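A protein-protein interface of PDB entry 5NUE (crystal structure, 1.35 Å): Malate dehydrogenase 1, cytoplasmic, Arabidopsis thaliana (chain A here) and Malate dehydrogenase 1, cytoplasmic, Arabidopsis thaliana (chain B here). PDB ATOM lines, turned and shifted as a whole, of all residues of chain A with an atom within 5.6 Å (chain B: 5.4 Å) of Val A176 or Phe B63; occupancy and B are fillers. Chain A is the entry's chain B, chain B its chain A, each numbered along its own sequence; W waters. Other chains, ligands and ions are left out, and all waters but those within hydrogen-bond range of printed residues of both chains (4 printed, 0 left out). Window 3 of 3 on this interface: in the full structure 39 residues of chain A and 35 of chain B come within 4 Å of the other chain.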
ATOM      1  N   ASN A 162      -4.793  22.402  29.093  1.00  0.00           N
ATOM      2  CA  ASN A 162      -6.257  22.375  29.078  1.00  0.00           C
ATOM      3  C   ASN A 162      -6.807  23.617  28.393  1.00  0.00           C
ATOM      4  O   ASN A 162      -7.831  23.538  27.699  1.00  0.00           O
ATOM      5  CB  ASN A 162      -6.784  22.204  30.525  1.00  0.00           C
ATOM      6  CG  ASN A 162      -6.514  20.796  31.076  1.00  0.00           C
ATOM      7  OD1 ASN A 162      -6.253  19.846  30.320  1.00  0.00           O
ATOM      8  ND2 ASN A 162      -6.660  20.632  32.379  1.00  0.00           N
ATOM      9  N   LEU A 165      -6.692  22.840  24.769  1.00  0.00           N
ATOM     10  CA  LEU A 165      -7.813  21.964  24.430  1.00  0.00           C
ATOM     11  C   LEU A 165      -9.113  22.757  24.327  1.00  0.00           C
ATOM     12  O   LEU A 165      -9.908  22.568  23.389  1.00  0.00           O
ATOM     13  CB  LEU A 165      -7.989  20.854  25.478  1.00  0.00           C
ATOM     14  CG  LEU A 165      -6.840  19.835  25.584  1.00  0.00           C
ATOM     15  CD1 LEU A 165      -7.144  18.927  26.759  1.00  0.00           C
ATOM     16  CD2 LEU A 165      -6.663  19.020  24.258  1.00  0.00           C
ATOM     17  N   GLY A 166      -9.361  23.633  25.316  1.00  0.00           N
ATOM     18  CA  GLY A 166     -10.574  24.429  25.327  1.00  0.00           C
ATOM     19  C   GLY A 166     -10.667  25.348  24.119  1.00  0.00           C
ATOM     20  O   GLY A 166     -11.734  25.480  23.503  1.00  0.00           O
ATOM     21  N   SER A 169     -11.722  23.138  21.150  1.00  0.00           N
ATOM     22  CA  SER A 169     -13.137  22.818  21.328  1.00  0.00           C
ATOM     23  C   SER A 169     -14.035  23.998  20.929  1.00  0.00           C
ATOM     24  O   SER A 169     -15.028  23.839  20.196  1.00  0.00           O
ATOM     25  CB  SER A 169     -13.349  22.498  22.816  1.00  0.00           C
ATOM     26  OG  SER A 169     -14.732  22.442  23.153  1.00  0.00           O
ATOM     27  N   VAL A 174     -16.918  21.543  19.057  1.00  0.00           N
ATOM     28  CA  VAL A 174     -17.024  20.128  19.416  1.00  0.00           C
ATOM     29  C   VAL A 174     -16.801  19.985  20.920  1.00  0.00           C
ATOM     30  O   VAL A 174     -16.115  20.823  21.524  1.00  0.00           O
ATOM     31  CB  VAL A 174     -15.988  19.286  18.661  1.00  0.00           C
ATOM     32  CG1 VAL A 174     -16.238  19.389  17.133  1.00  0.00           C
ATOM     33  CG2 VAL A 174     -14.590  19.743  19.002  1.00  0.00           C
ATOM     34  N   PRO A 175     -17.321  18.938  21.555  1.00  0.00           N
ATOM     35  CA  PRO A 175     -17.080  18.762  22.991  1.00  0.00           C
ATOM     36  C   PRO A 175     -15.599  18.582  23.265  1.00  0.00           C
ATOM     37  O   PRO A 175     -14.890  17.888  22.534  1.00  0.00           O
ATOM     38  CB  PRO A 175     -17.843  17.480  23.329  1.00  0.00           C
ATOM     39  CG  PRO A 175     -18.761  17.214  22.173  1.00  0.00           C
ATOM     40  CD  PRO A 175     -18.174  17.877  20.975  1.00  0.00           C
ATOM     41  N   VAL A 176     -15.139  19.202  24.352  1.00  0.00           N
ATOM     42  CA  VAL A 176     -13.720  19.110  24.697  1.00  0.00           C
ATOM     43  C   VAL A 176     -13.308  17.679  25.004  1.00  0.00           C
ATOM     44  O   VAL A 176     -12.136  17.328  24.835  1.00  0.00           O
ATOM     45  CB  VAL A 176     -13.332  20.087  25.823  1.00  0.00           C
ATOM     46  CG1 VAL A 176     -13.901  19.584  27.209  1.00  0.00           C
ATOM     47  CG2 VAL A 176     -11.797  20.272  25.843  1.00  0.00           C
ATOM     48  N   SER A 177     -14.256  16.823  25.389  1.00  0.00           N
ATOM     49  CA  SER A 177     -13.967  15.404  25.604  1.00  0.00           C
ATOM     50  C   SER A 177     -13.449  14.724  24.347  1.00  0.00           C
ATOM     51  O   SER A 177     -12.785  13.685  24.451  1.00  0.00           O
ATOM     52  CB  SER A 177     -15.242  14.687  26.075  1.00  0.00           C
ATOM     53  OG  SER A 177     -16.272  14.878  25.117  1.00  0.00           O
ATOM     54  N   ASP A 178     -13.711  15.290  23.181  1.00  0.00           N
ATOM     55  CA  ASP A 178     -13.273  14.719  21.914  1.00  0.00           C
ATOM     56  C   ASP A 178     -11.899  15.202  21.465  1.00  0.00           C
ATOM     57  O   ASP A 178     -11.393  14.705  20.446  1.00  0.00           O
ATOM     58  CB  ASP A 178     -14.288  15.054  20.812  1.00  0.00           C
ATOM     59  CG  ASP A 178     -15.517  14.193  20.884  1.00  0.00           C
ATOM     60  OD1 ASP A 178     -15.417  13.039  21.376  1.00  0.00           O
ATOM     61  OD2 ASP A 178     -16.571  14.675  20.456  1.00  0.00           O
ATOM     62  N   VAL A 179     -11.280  16.141  22.180  1.00  0.00           N
ATOM     63  CA  VAL A 179     -10.036  16.761  21.751  1.00  0.00           C
ATOM     64  C   VAL A 179      -8.921  16.234  22.642  1.00  0.00           C
ATOM     65  O   VAL A 179      -9.059  16.208  23.876  1.00  0.00           O
ATOM     66  CB  VAL A 179     -10.106  18.306  21.855  1.00  0.00           C
ATOM     67  CG1 VAL A 179      -8.849  18.943  21.240  1.00  0.00           C
ATOM     68  CG2 VAL A 179     -11.362  18.868  21.185  1.00  0.00           C
ATOM     69  N   LYS A 180      -7.778  15.878  22.039  1.00  0.00           N
ATOM     70  CA  LYS A 180      -6.636  15.395  22.826  1.00  0.00           C
ATOM     71  C   LYS A 180      -5.306  15.745  22.161  1.00  0.00           C
ATOM     72  O   LYS A 180      -5.234  16.065  20.972  1.00  0.00           O
ATOM     73  CB  LYS A 180      -6.669  13.883  23.051  1.00  0.00           C
ATOM     74  CG  LYS A 180      -6.457  13.107  21.766  1.00  0.00           C
ATOM     75  CD  LYS A 180      -6.569  11.644  22.026  1.00  0.00           C
ATOM     76  CE  LYS A 180      -6.346  10.902  20.695  1.00  0.00           C
ATOM     77  NZ  LYS A 180      -6.450   9.439  20.793  1.00  0.00           N
ATOM     78  N   LEU A 245     -10.122  28.367  39.871  1.00  0.00           N
ATOM     79  CA  LEU A 245     -10.938  27.201  39.564  1.00  0.00           C
ATOM     80  C   LEU A 245     -10.209  26.297  38.557  1.00  0.00           C
ATOM     81  O   LEU A 245     -10.117  25.070  38.732  1.00  0.00           O
ATOM     82  CB  LEU A 245     -12.280  27.711  38.996  1.00  0.00           C
ATOM     83  CG  LEU A 245     -13.357  26.910  38.330  1.00  0.00           C
ATOM     84  CD1 LEU A 245     -14.518  27.848  38.070  1.00  0.00           C
ATOM     85  CD2 LEU A 245     -12.949  26.218  37.017  1.00  0.00           C
ATOM     86  N   SER A 249      -8.409  22.607  39.116  1.00  0.00           N
ATOM     87  CA  SER A 249      -8.868  21.459  38.349  1.00  0.00           C
ATOM     88  C   SER A 249      -7.713  20.846  37.559  1.00  0.00           C
ATOM     89  O   SER A 249      -7.579  19.619  37.473  1.00  0.00           O
ATOM     90  CB  SER A 249      -9.995  21.905  37.416  1.00  0.00           C
ATOM     91  OG  SER A 249     -10.521  20.795  36.742  1.00  0.00           O
ATOM     92  N   PRO B  23     -17.471  24.334  39.173  1.00  0.00           N
ATOM     93  CA  PRO B  23     -16.555  23.246  38.788  1.00  0.00           C
ATOM     94  C   PRO B  23     -16.973  21.919  39.389  1.00  0.00           C
ATOM     95  O   PRO B  23     -16.659  20.861  38.811  1.00  0.00           O
ATOM     96  CB  PRO B  23     -15.190  23.717  39.308  1.00  0.00           C
ATOM     97  CG  PRO B  23     -15.530  24.585  40.536  1.00  0.00           C
ATOM     98  CD  PRO B  23     -16.833  25.277  40.127  1.00  0.00           C
ATOM     99  N   ALA B  26     -19.470  20.638  36.945  1.00  0.00           N
ATOM    100  CA  ALA B  26     -18.824  20.212  35.711  1.00  0.00           C
ATOM    101  C   ALA B  26     -18.039  18.913  35.892  1.00  0.00           C
ATOM    102  O   ALA B  26     -17.815  18.195  34.908  1.00  0.00           O
ATOM    103  CB  ALA B  26     -17.885  21.320  35.257  1.00  0.00           C
ATOM    104  N   ARG B  27     -17.582  18.618  37.103  1.00  0.00           N
ATOM    105  CA  ARG B  27     -16.824  17.404  37.412  1.00  0.00           C
ATOM    106  C   ARG B  27     -17.707  16.190  37.629  1.00  0.00           C
ATOM    107  O   ARG B  27     -17.187  15.081  37.772  1.00  0.00           O
ATOM    108  CB  ARG B  27     -15.997  17.601  38.684  1.00  0.00           C
ATOM    109  CG  ARG B  27     -14.699  18.290  38.462  1.00  0.00           C
ATOM    110  CD  ARG B  27     -13.738  17.430  37.667  1.00  0.00           C
ATOM    111  NE  ARG B  27     -12.406  18.032  37.586  1.00  0.00           N
ATOM    112  CZ  ARG B  27     -11.387  17.469  36.922  1.00  0.00           C
ATOM    113  NH1 ARG B  27     -11.584  16.334  36.246  1.00  0.00           N
ATOM    114  NH2 ARG B  27     -10.178  18.039  36.894  1.00  0.00           N
ATOM    115  N   GLU B  57     -12.890  30.334  32.484  1.00  0.00           N
ATOM    116  CA  GLU B  57     -12.185  29.319  33.263  1.00  0.00           C
ATOM    117  C   GLU B  57     -12.810  27.936  33.127  1.00  0.00           C
ATOM    118  O   GLU B  57     -12.083  26.924  33.198  1.00  0.00           O
ATOM    119  CB  GLU B  57     -12.121  29.703  34.743  1.00  0.00           C
ATOM    120  CG  GLU B  57     -11.143  30.834  35.056  1.00  0.00           C
ATOM    121  CD  GLU B  57     -10.701  30.761  36.517  1.00  0.00           C
ATOM    122  OE1 GLU B  57      -9.959  29.807  36.895  1.00  0.00           O
ATOM    123  OE2 GLU B  57     -11.096  31.664  37.303  1.00  0.00           O
ATOM    124  N   LEU B  58     -14.134  27.854  33.003  1.00  0.00           N
ATOM    125  CA  LEU B  58     -14.786  26.564  32.802  1.00  0.00           C
ATOM    126  C   LEU B  58     -14.310  25.948  31.495  1.00  0.00           C
ATOM    127  O   LEU B  58     -14.030  24.745  31.428  1.00  0.00           O
ATOM    128  CB  LEU B  58     -16.322  26.715  32.768  1.00  0.00           C
ATOM    129  CG  LEU B  58     -16.967  26.938  34.165  1.00  0.00           C
ATOM    130  CD1 LEU B  58     -18.422  27.401  34.027  1.00  0.00           C
ATOM    131  CD2 LEU B  58     -16.852  25.694  35.090  1.00  0.00           C
ATOM    132  N   ILE B  59     -14.219  26.759  30.438  1.00  0.00           N
ATOM    133  CA  ILE B  59     -13.631  26.292  29.174  1.00  0.00           C
ATOM    134  C   ILE B  59     -12.168  25.876  29.357  1.00  0.00           C
ATOM    135  O   ILE B  59     -11.723  24.844  28.812  1.00  0.00           O
ATOM    136  CB  ILE B  59     -13.799  27.390  28.112  1.00  0.00           C
ATOM    137  CG1 ILE B  59     -15.267  27.502  27.726  1.00  0.00           C
ATOM    138  CG2 ILE B  59     -12.913  27.093  26.878  1.00  0.00           C
ATOM    139  CD1 ILE B  59     -15.573  28.816  26.988  1.00  0.00           C
ATOM    140  N   ALA B  61     -10.629  24.669  31.844  1.00  0.00           N
ATOM    141  CA  ALA B  61     -10.436  23.461  32.627  1.00  0.00           C
ATOM    142  C   ALA B  61     -10.621  22.185  31.812  1.00  0.00           C
ATOM    143  O   ALA B  61     -10.268  21.098  32.287  1.00  0.00           O
ATOM    144  CB  ALA B  61     -11.372  23.471  33.848  1.00  0.00           C
ATOM    145  N   ALA B  62     -11.186  22.280  30.606  1.00  0.00           N
ATOM    146  CA  ALA B  62     -11.341  21.092  29.728  1.00  0.00           C
ATOM    147  C   ALA B  62     -12.072  19.961  30.466  1.00  0.00           C
ATOM    148  O   ALA B  62     -11.611  18.813  30.544  1.00  0.00           O
ATOM    149  CB  ALA B  62      -9.985  20.615  29.155  1.00  0.00           C
ATOM    150  N   PHE B  63     -13.235  20.292  31.012  1.00  0.00           N
ATOM    151  CA  PHE B  63     -14.044  19.314  31.755  1.00  0.00           C
ATOM    152  C   PHE B  63     -14.757  18.407  30.774  1.00  0.00           C
ATOM    153  O   PHE B  63     -15.638  18.882  30.048  1.00  0.00           O
ATOM    154  CB  PHE B  63     -15.138  20.010  32.603  1.00  0.00           C
ATOM    155  CG  PHE B  63     -14.630  20.726  33.814  1.00  0.00           C
ATOM    156  CD1 PHE B  63     -14.041  20.019  34.877  1.00  0.00           C
ATOM    157  CD2 PHE B  63     -14.793  22.107  33.945  1.00  0.00           C
ATOM    158  CE1 PHE B  63     -13.603  20.688  36.014  1.00  0.00           C
ATOM    159  CE2 PHE B  63     -14.368  22.790  35.087  1.00  0.00           C
ATOM    160  CZ  PHE B  63     -13.763  22.094  36.125  1.00  0.00           C
ATOM    161  N   PRO B  64     -14.458  17.106  30.752  1.00  0.00           N
ATOM    162  CA  PRO B  64     -15.058  16.252  29.701  1.00  0.00           C
ATOM    163  C   PRO B  64     -16.575  16.094  29.823  1.00  0.00           C
ATOM    164  O   PRO B  64     -17.239  15.884  28.800  1.00  0.00           O
ATOM    165  CB  PRO B  64     -14.344  14.906  29.892  1.00  0.00           C
ATOM    166  CG  PRO B  64     -13.765  14.970  31.287  1.00  0.00           C
ATOM    167  CD  PRO B  64     -13.431  16.392  31.533  1.00  0.00           C
ATOM    168  N   LEU B  65     -17.148  16.217  31.029  1.00  0.00           N
ATOM    169  CA  LEU B  65     -18.590  16.057  31.158  1.00  0.00           C
ATOM    170  C   LEU B  65     -19.349  17.299  30.750  1.00  0.00           C
ATOM    171  O   LEU B  65     -20.572  17.238  30.571  1.00  0.00           O
ATOM    172  CB  LEU B  65     -19.011  15.738  32.600  1.00  0.00           C
ATOM    173  CG  LEU B  65     -18.678  14.318  33.097  1.00  0.00           C
ATOM    174  CD1 LEU B  65     -19.063  14.163  34.552  1.00  0.00           C
ATOM    175  CD2 LEU B  65     -19.382  13.270  32.234  1.00  0.00           C
ATOM    176  N   LEU B  66     -18.670  18.423  30.620  1.00  0.00           N
ATOM    177  CA  LEU B  66     -19.343  19.692  30.377  1.00  0.00           C
ATOM    178  C   LEU B  66     -19.549  19.878  28.877  1.00  0.00           C
ATOM    179  O   LEU B  66     -18.584  19.865  28.112  1.00  0.00           O
ATOM    180  CB  LEU B  66     -18.476  20.810  30.963  1.00  0.00           C
ATOM    181  CG  LEU B  66     -19.040  22.232  30.844  1.00  0.00           C
ATOM    182  CD1 LEU B  66     -20.409  22.309  31.553  1.00  0.00           C
ATOM    183  CD2 LEU B  66     -18.023  23.201  31.479  1.00  0.00           C
HETATM  184  O   HOH W   1      -9.023  20.793  34.609  1.00  0.00           O
HETATM  185  O   HOH W   2     -17.011  17.601  26.622  1.00  0.00           O
HETATM  186  O   HOH W   3     -16.985  20.892  25.774  1.00  0.00           O
HETATM  187  O   HOH W   4     -11.893  19.938  39.428  1.00  0.00           O
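Water W1 lies within hydrogen-bond range of OG of Ser A249 (2.6 Å), O of Ala B61 (2.7 Å) and ND2 of Asn A162 (3.3 Å).
Water W4 lies within hydrogen-bond range of the guanidinium group (NE) of Arg B27 and the side-chain hydroxyl (OG) of Ser A249.
Water W2 lies within hydrogen-bond range of O of Pro B64 (2.8 Å), N of Ser A177 (3.1 Å), O of Leu B66 (3.1 Å) and N of Val A176 (3.3 Å).
Water W3 lies within hydrogen-bond range of the backbone NH of Val A176 (2.9 Å) and the backbone carbonyl oxygen of Leu B66 (3.0 Å).
Among the printed residues, pairs that only touch across the chains: Ser A249 with Phe B63, Val A176 with Phe B63, Ser A177 with Pro B64, Asn A162 with Ala B61, Gly A166 with Ile B59, Val A176 with Ala B62, Leu A245 with Pro B23 and Asn A162 with Ala B62.
Of the printed residues of chain B, Asn A162 touches Ala B61 and Ala B62.
Pro A175 touches none of the printed residues of chain B.
Val A176 touches just these residues of chain B: Ala B62 (3.8 Å) and Phe B63 (3.4 Å).
Of the printed residues of chain B, Ser A249 touches Arg B27 and Phe B63.
Ala B26 touches none of the printed residues of chain A.
Printed residues of chain A within 4 Å of Glu B57: Leu A245.
Printed residues of chain A within 4 Å of Phe B63: Val A176 and Ser A249.
The nearest residue of chain B that does not touch Val A176 is Pro B64 (4.3 Å).
The nearest printed residue of chain A that does not touch Phe B63 is Leu A245 (4.2 Å).
The nearest printed residue of chain A that does not touch Arg B27 is Asn A162 (6.3 Å).
Hydrophobic or aromatic side chains of chain B within 4 Å of the printed part of chain A: Pro B23, Ile B59, Ala B62, Phe B63 and Pro B64.
Along chain B the printed residues that touch a printed residue of chain A span positions 23 to 64.
Hydrophobic or aromatic side chains of chain A within 4 Å of the printed part of chain B: Val A176 and Leu A245.
Among the printed residues, 10 pairs touch across the chains.
OG of Ser A169 lies within hydrogen-bond range of N of Val A176, 3.5 Å away.
The backbone NH (N) of Leu A245 lies within hydrogen-bond range of the side-chain carboxylate (OE1) of Glu B57 (3.3 Å).
The guanidinium group of Arg B27 lies within hydrogen-bond range of the side-chain hydroxyl of Ser A249, at 2.8 Å.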
